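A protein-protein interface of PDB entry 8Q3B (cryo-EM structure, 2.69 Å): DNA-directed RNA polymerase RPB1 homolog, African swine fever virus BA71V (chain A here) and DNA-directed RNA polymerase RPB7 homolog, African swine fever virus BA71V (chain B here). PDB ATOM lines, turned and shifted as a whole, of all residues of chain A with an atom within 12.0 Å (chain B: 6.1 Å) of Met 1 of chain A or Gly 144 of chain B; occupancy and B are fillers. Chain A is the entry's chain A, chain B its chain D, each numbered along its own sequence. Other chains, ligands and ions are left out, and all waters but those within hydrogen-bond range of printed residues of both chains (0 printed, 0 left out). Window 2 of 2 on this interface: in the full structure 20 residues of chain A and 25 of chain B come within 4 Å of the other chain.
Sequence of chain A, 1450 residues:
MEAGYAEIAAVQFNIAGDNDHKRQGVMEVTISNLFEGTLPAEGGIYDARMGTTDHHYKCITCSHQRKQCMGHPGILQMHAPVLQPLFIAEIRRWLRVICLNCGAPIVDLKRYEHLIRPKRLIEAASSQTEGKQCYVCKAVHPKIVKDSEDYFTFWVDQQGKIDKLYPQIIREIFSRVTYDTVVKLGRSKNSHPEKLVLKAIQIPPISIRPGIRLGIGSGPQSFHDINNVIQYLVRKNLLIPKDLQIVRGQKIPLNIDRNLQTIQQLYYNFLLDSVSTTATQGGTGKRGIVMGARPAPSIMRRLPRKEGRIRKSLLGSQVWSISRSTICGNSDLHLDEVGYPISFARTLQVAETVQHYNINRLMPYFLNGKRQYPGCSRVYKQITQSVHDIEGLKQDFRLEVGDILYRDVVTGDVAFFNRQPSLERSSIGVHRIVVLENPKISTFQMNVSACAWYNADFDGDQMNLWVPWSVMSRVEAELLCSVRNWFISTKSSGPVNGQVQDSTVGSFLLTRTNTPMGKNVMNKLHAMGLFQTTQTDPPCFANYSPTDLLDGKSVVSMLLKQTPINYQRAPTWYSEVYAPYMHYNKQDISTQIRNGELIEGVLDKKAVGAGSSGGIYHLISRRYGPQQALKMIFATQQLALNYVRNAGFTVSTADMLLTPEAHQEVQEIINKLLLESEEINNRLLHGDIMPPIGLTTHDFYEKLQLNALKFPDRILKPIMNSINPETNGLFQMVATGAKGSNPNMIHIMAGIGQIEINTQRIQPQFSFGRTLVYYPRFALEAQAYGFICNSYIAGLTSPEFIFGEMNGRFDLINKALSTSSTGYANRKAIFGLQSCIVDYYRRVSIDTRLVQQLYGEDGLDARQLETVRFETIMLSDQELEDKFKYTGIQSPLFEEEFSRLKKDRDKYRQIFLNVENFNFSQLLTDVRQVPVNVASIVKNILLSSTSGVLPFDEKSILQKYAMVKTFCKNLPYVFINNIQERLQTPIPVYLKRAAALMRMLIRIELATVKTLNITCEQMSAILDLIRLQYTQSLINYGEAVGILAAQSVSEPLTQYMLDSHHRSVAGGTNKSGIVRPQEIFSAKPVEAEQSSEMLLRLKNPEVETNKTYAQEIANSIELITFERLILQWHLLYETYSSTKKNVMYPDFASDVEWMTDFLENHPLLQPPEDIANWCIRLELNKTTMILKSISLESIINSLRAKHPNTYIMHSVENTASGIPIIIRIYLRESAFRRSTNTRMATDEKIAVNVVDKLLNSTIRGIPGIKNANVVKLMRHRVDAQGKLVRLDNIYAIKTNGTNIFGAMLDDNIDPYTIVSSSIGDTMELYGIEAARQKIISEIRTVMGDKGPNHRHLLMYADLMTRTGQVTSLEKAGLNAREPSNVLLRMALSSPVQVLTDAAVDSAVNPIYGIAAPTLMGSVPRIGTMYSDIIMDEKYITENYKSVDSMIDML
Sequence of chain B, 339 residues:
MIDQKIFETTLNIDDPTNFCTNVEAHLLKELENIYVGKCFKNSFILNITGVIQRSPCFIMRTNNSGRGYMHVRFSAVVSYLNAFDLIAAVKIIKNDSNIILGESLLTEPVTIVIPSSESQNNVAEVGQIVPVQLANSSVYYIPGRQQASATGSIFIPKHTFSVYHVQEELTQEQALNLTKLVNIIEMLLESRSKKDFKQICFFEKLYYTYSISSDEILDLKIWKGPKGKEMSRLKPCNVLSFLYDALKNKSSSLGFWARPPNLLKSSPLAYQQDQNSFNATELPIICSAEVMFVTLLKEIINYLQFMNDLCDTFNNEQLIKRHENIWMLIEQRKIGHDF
O of Cys 39 of chain B sits at hydrogen-bond distance from N of Gly 144 of chain B.
Hydrophobic or aromatic side chains of chain A within 4 Å of the printed part of chain B: Met 1. Of the 11 printed residues of chain B, 4 touch a printed residue of chain A. Printed residues of chain B that touch a printed residue of chain A: Tyr 35, Lys 38, Phe 40 and Gly 144. Hydrophobic or aromatic side chains of chain B within 4 Å of the printed part of chain A: Tyr 35 and Phe 40. Along chain B the printed residues that touch a printed residue of chain A span positions 35 to 144. Among the printed residues, no Asp or Glu carboxylate lies within 4 Å of a Lys or Arg side-chain nitrogen of the other chain.
Met 1 of chain A touches Tyr 35 of chain B. CD of Lys 38 of chain B touches N of Met 1 of chain A, at 3.8 Å. SD of Met 1 of chain A touches CD1 of Phe 40 of chain B, 3.9 Å away. Met 1 of chain A touches Gly 144 of chain B.
Printed residues of chain B within 4 Å of Met 1 of chain A: Tyr 35 (3.4 Å), Lys 38 (3.8 Å), Phe 40 (3.9 Å) and Gly 144 (3.5 Å). Glu 2 of chain A touches none of the printed residues of chain B. Tyr 5 of chain A touches none of the printed residues of chain B. No residue of chain A comes within 4 Å of Ile 34 of chain B. Printed residues of chain A within 4 Å of Tyr 35 of chain B: Met 1 (3.4 Å). Lys 38 of chain B touches just one residue of chain A: Met 1 (3.8 Å). No residue of chain A comes within 4 Å of Cys 39 of chain B. Gly 144 of chain B touches just one residue of chain A: Met 1. No residue of chain A comes within 4 Å of Arg 145 of chain B. The nearest residue of chain A that does not touch Gly 144 of chain B is Glu 2 of chain A (8.0 Å).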
ATOM      1  N   MET A   1      -8.887  14.913   3.680  1.00  0.00           N
ATOM      2  CA  MET A   1      -8.741  14.264   2.345  1.00  0.00           C
ATOM      3  C   MET A   1      -9.669  14.914   1.330  1.00  0.00           C
ATOM      4  O   MET A   1     -10.739  15.407   1.681  1.00  0.00           O
ATOM      5  CB  MET A   1      -9.044  12.769   2.429  1.00  0.00           C
ATOM      6  CG  MET A   1      -8.135  11.989   3.357  1.00  0.00           C
ATOM      7  SD  MET A   1      -6.807  11.136   2.487  1.00  0.00           S
ATOM      8  CE  MET A   1      -5.497  12.350   2.596  1.00  0.00           C
ATOM      9  N   GLU A   2      -9.252  14.909   0.066  1.00  0.00           N
ATOM     10  CA  GLU A   2     -10.066  15.428  -1.021  1.00  0.00           C
ATOM     11  C   GLU A   2      -9.938  14.508  -2.224  1.00  0.00           C
ATOM     12  O   GLU A   2      -8.906  13.862  -2.425  1.00  0.00           O
ATOM     13  CB  GLU A   2      -9.656  16.855  -1.405  1.00  0.00           C
ATOM     14  CG  GLU A   2      -9.632  17.828  -0.234  1.00  0.00           C
ATOM     15  CD  GLU A   2     -10.092  19.224  -0.612  1.00  0.00           C
ATOM     16  OE1 GLU A   2     -10.302  19.486  -1.815  1.00  0.00           O
ATOM     17  OE2 GLU A   2     -10.242  20.065   0.300  1.00  0.00           O
ATOM     18  N   ALA A   3     -10.999  14.457  -3.025  1.00  0.00           N
ATOM     19  CA  ALA A   3     -11.035  13.649  -4.237  1.00  0.00           C
ATOM     20  C   ALA A   3     -10.724  14.556  -5.420  1.00  0.00           C
ATOM     21  O   ALA A   3     -11.529  15.422  -5.775  1.00  0.00           O
ATOM     22  CB  ALA A   3     -12.395  12.975  -4.400  1.00  0.00           C
ATOM     23  N   GLY A   4      -9.558  14.357  -6.025  1.00  0.00           N
ATOM     24  CA  GLY A   4      -9.149  15.202  -7.125  1.00  0.00           C
ATOM     25  C   GLY A   4      -9.962  14.956  -8.379  1.00  0.00           C
ATOM     26  O   GLY A   4     -10.545  13.894  -8.590  1.00  0.00           O
ATOM     27  N   TYR A   5      -9.992  15.975  -9.233  1.00  0.00           N
ATOM     28  CA  TYR A   5     -10.720  15.880 -10.489  1.00  0.00           C
ATOM     29  C   TYR A   5     -10.141  14.769 -11.355  1.00  0.00           C
ATOM     30  O   TYR A   5      -8.922  14.595 -11.438  1.00  0.00           O
ATOM     31  CB  TYR A   5     -10.660  17.221 -11.222  1.00  0.00           C
ATOM     32  CG  TYR A   5     -11.161  17.186 -12.645  1.00  0.00           C
ATOM     33  CD1 TYR A   5     -12.494  17.428 -12.939  1.00  0.00           C
ATOM     34  CD2 TYR A   5     -10.296  16.932 -13.699  1.00  0.00           C
ATOM     35  CE1 TYR A   5     -12.951  17.405 -14.238  1.00  0.00           C
ATOM     36  CE2 TYR A   5     -10.746  16.906 -14.999  1.00  0.00           C
ATOM     37  CZ  TYR A   5     -12.072  17.144 -15.264  1.00  0.00           C
ATOM     38  OH  TYR A   5     -12.519  17.120 -16.562  1.00  0.00           O
ATOM     39  N   HIS A  64     -25.077  10.252   3.110  1.00  0.00           N
ATOM     40  CA  HIS A  64     -25.638  11.212   2.172  1.00  0.00           C
ATOM     41  C   HIS A  64     -27.156  11.090   2.171  1.00  0.00           C
ATOM     42  O   HIS A  64     -27.726  10.096   2.629  1.00  0.00           O
ATOM     43  CB  HIS A  64     -25.090  10.994   0.754  1.00  0.00           C
ATOM     44  CG  HIS A  64     -23.737  11.594   0.529  1.00  0.00           C
ATOM     45  ND1 HIS A  64     -23.493  12.945   0.651  1.00  0.00           N
ATOM     46  CD2 HIS A  64     -22.558  11.028   0.180  1.00  0.00           C
ATOM     47  CE1 HIS A  64     -22.220  13.185   0.391  1.00  0.00           C
ATOM     48  NE2 HIS A  64     -21.631  12.039   0.103  1.00  0.00           N
ATOM     49  N   ILE B  34      -3.875  19.404   3.196  1.00  0.00           N
ATOM     50  CA  ILE B  34      -4.715  18.265   2.841  1.00  0.00           C
ATOM     51  C   ILE B  34      -4.166  16.960   3.403  1.00  0.00           C
ATOM     52  O   ILE B  34      -4.915  16.156   3.965  1.00  0.00           O
ATOM     53  CB  ILE B  34      -4.874  18.197   1.307  1.00  0.00           C
ATOM     54  CG1 ILE B  34      -5.702  19.389   0.822  1.00  0.00           C
ATOM     55  CG2 ILE B  34      -5.523  16.877   0.891  1.00  0.00           C
ATOM     56  CD1 ILE B  34      -5.895  19.450  -0.676  1.00  0.00           C
ATOM     57  N   TYR B  35      -2.862  16.716   3.271  1.00  0.00           N
ATOM     58  CA  TYR B  35      -2.318  15.387   3.519  1.00  0.00           C
ATOM     59  C   TYR B  35      -1.570  15.250   4.838  1.00  0.00           C
ATOM     60  O   TYR B  35      -1.502  14.138   5.372  1.00  0.00           O
ATOM     61  CB  TYR B  35      -1.384  14.985   2.371  1.00  0.00           C
ATOM     62  CG  TYR B  35      -2.134  14.621   1.114  1.00  0.00           C
ATOM     63  CD1 TYR B  35      -2.675  13.355   0.949  1.00  0.00           C
ATOM     64  CD2 TYR B  35      -2.322  15.549   0.102  1.00  0.00           C
ATOM     65  CE1 TYR B  35      -3.370  13.020  -0.193  1.00  0.00           C
ATOM     66  CE2 TYR B  35      -3.016  15.224  -1.045  1.00  0.00           C
ATOM     67  CZ  TYR B  35      -3.539  13.958  -1.186  1.00  0.00           C
ATOM     68  OH  TYR B  35      -4.232  13.628  -2.327  1.00  0.00           O
ATOM     69  N   GLY B  37      -0.785  14.854   8.547  1.00  0.00           N
ATOM     70  CA  GLY B  37      -1.582  14.427   9.678  1.00  0.00           C
ATOM     71  C   GLY B  37      -2.700  13.469   9.345  1.00  0.00           C
ATOM     72  O   GLY B  37      -3.661  13.370  10.113  1.00  0.00           O
ATOM     73  N   LYS B  38      -2.611  12.761   8.222  1.00  0.00           N
ATOM     74  CA  LYS B  38      -3.637  11.811   7.819  1.00  0.00           C
ATOM     75  C   LYS B  38      -2.974  10.572   7.237  1.00  0.00           C
ATOM     76  O   LYS B  38      -1.843  10.618   6.746  1.00  0.00           O
ATOM     77  CB  LYS B  38      -4.601  12.424   6.796  1.00  0.00           C
ATOM     78  CG  LYS B  38      -5.619  13.376   7.403  1.00  0.00           C
ATOM     79  CD  LYS B  38      -6.271  14.255   6.346  1.00  0.00           C
ATOM     80  CE  LYS B  38      -6.236  15.724   6.737  1.00  0.00           C
ATOM     81  NZ  LYS B  38      -6.813  15.967   8.088  1.00  0.00           N
ATOM     82  N   CYS B  39      -3.697   9.458   7.297  1.00  0.00           N
ATOM     83  CA  CYS B  39      -3.225   8.194   6.748  1.00  0.00           C
ATOM     84  C   CYS B  39      -3.572   8.126   5.267  1.00  0.00           C
ATOM     85  O   CYS B  39      -4.725   8.345   4.883  1.00  0.00           O
ATOM     86  CB  CYS B  39      -3.851   7.015   7.491  1.00  0.00           C
ATOM     87  SG  CYS B  39      -3.053   6.618   9.061  1.00  0.00           S
ATOM     88  N   PHE B  40      -2.572   7.833   4.439  1.00  0.00           N
ATOM     89  CA  PHE B  40      -2.762   7.753   2.997  1.00  0.00           C
ATOM     90  C   PHE B  40      -1.879   6.656   2.427  1.00  0.00           C
ATOM     91  O   PHE B  40      -0.684   6.599   2.731  1.00  0.00           O
ATOM     92  CB  PHE B  40      -2.439   9.092   2.323  1.00  0.00           C
ATOM     93  CG  PHE B  40      -2.855   9.163   0.883  1.00  0.00           C
ATOM     94  CD1 PHE B  40      -4.175   8.957   0.518  1.00  0.00           C
ATOM     95  CD2 PHE B  40      -1.928   9.433  -0.106  1.00  0.00           C
ATOM     96  CE1 PHE B  40      -4.558   9.021  -0.805  1.00  0.00           C
ATOM     97  CE2 PHE B  40      -2.307   9.499  -1.431  1.00  0.00           C
ATOM     98  CZ  PHE B  40      -3.623   9.292  -1.781  1.00  0.00           C
ATOM     99  N   ILE B 142      -6.186   3.094   7.948  1.00  0.00           N
ATOM    100  CA  ILE B 142      -7.414   3.467   7.237  1.00  0.00           C
ATOM    101  C   ILE B 142      -7.215   4.832   6.591  1.00  0.00           C
ATOM    102  O   ILE B 142      -6.846   5.797   7.291  1.00  0.00           O
ATOM    103  CB  ILE B 142      -8.611   3.487   8.201  1.00  0.00           C
ATOM    104  CG1 ILE B 142      -8.780   2.122   8.869  1.00  0.00           C
ATOM    105  CG2 ILE B 142      -9.885   3.876   7.459  1.00  0.00           C
ATOM    106  CD1 ILE B 142      -9.769   2.118  10.015  1.00  0.00           C
ATOM    107  N   PRO B 143      -7.436   4.986   5.286  1.00  0.00           N
ATOM    108  CA  PRO B 143      -7.213   6.296   4.664  1.00  0.00           C
ATOM    109  C   PRO B 143      -8.103   7.366   5.278  1.00  0.00           C
ATOM    110  O   PRO B 143      -9.277   7.133   5.572  1.00  0.00           O
ATOM    111  CB  PRO B 143      -7.554   6.055   3.188  1.00  0.00           C
ATOM    112  CG  PRO B 143      -8.388   4.825   3.175  1.00  0.00           C
ATOM    113  CD  PRO B 143      -7.904   3.989   4.310  1.00  0.00           C
ATOM    114  N   GLY B 144      -7.528   8.552   5.468  1.00  0.00           N
ATOM    115  CA  GLY B 144      -8.244   9.690   5.991  1.00  0.00           C
ATOM    116  C   GLY B 144      -8.237   9.818   7.500  1.00  0.00           C
ATOM    117  O   GLY B 144      -8.556  10.894   8.016  1.00  0.00           O
ATOM    118  N   ARG B 145      -7.885   8.759   8.223  1.00  0.00           N
ATOM    119  CA  ARG B 145      -7.833   8.831   9.673  1.00  0.00           C
ATOM    120  C   ARG B 145      -6.558   9.530  10.124  1.00  0.00           C
ATOM    121  O   ARG B 145      -5.496   9.393   9.511  1.00  0.00           O
ATOM    122  CB  ARG B 145      -7.910   7.433  10.288  1.00  0.00           C
ATOM    123  CG  ARG B 145      -9.165   6.662   9.914  1.00  0.00           C
ATOM    124  CD  ARG B 145     -10.404   7.265  10.556  1.00  0.00           C
ATOM    125  NE  ARG B 145     -11.621   6.575  10.144  1.00  0.00           N
ATOM    126  CZ  ARG B 145     -12.110   5.493  10.734  1.00  0.00           C
ATOM    127  NH1 ARG B 145     -11.505   4.934  11.770  1.00  0.00           N
ATOM    128  NH2 ARG B 145     -13.235   4.954  10.271  1.00  0.00           N
ATOM    129  N   GLN B 146      -6.674  10.285  11.214  1.00  0.00           N
ATOM    130  CA  GLN B 146      -5.556  11.060  11.735  1.00  0.00           C
ATOM    131  C   GLN B 146      -4.638  10.245  12.635  1.00  0.00           C
ATOM    132  O   GLN B 146      -3.647  10.789  13.133  1.00  0.00           O
ATOM    133  CB  GLN B 146      -6.077  12.280  12.497  1.00  0.00           C
ATOM    134  CG  GLN B 146      -6.994  13.168  11.672  1.00  0.00           C
ATOM    135  CD  GLN B 146      -7.474  14.382  12.439  1.00  0.00           C
ATOM    136  OE1 GLN B 146      -7.061  14.619  13.573  1.00  0.00           O
ATOM    137  NE2 GLN B 146      -8.353  15.162  11.820  1.00  0.00           N
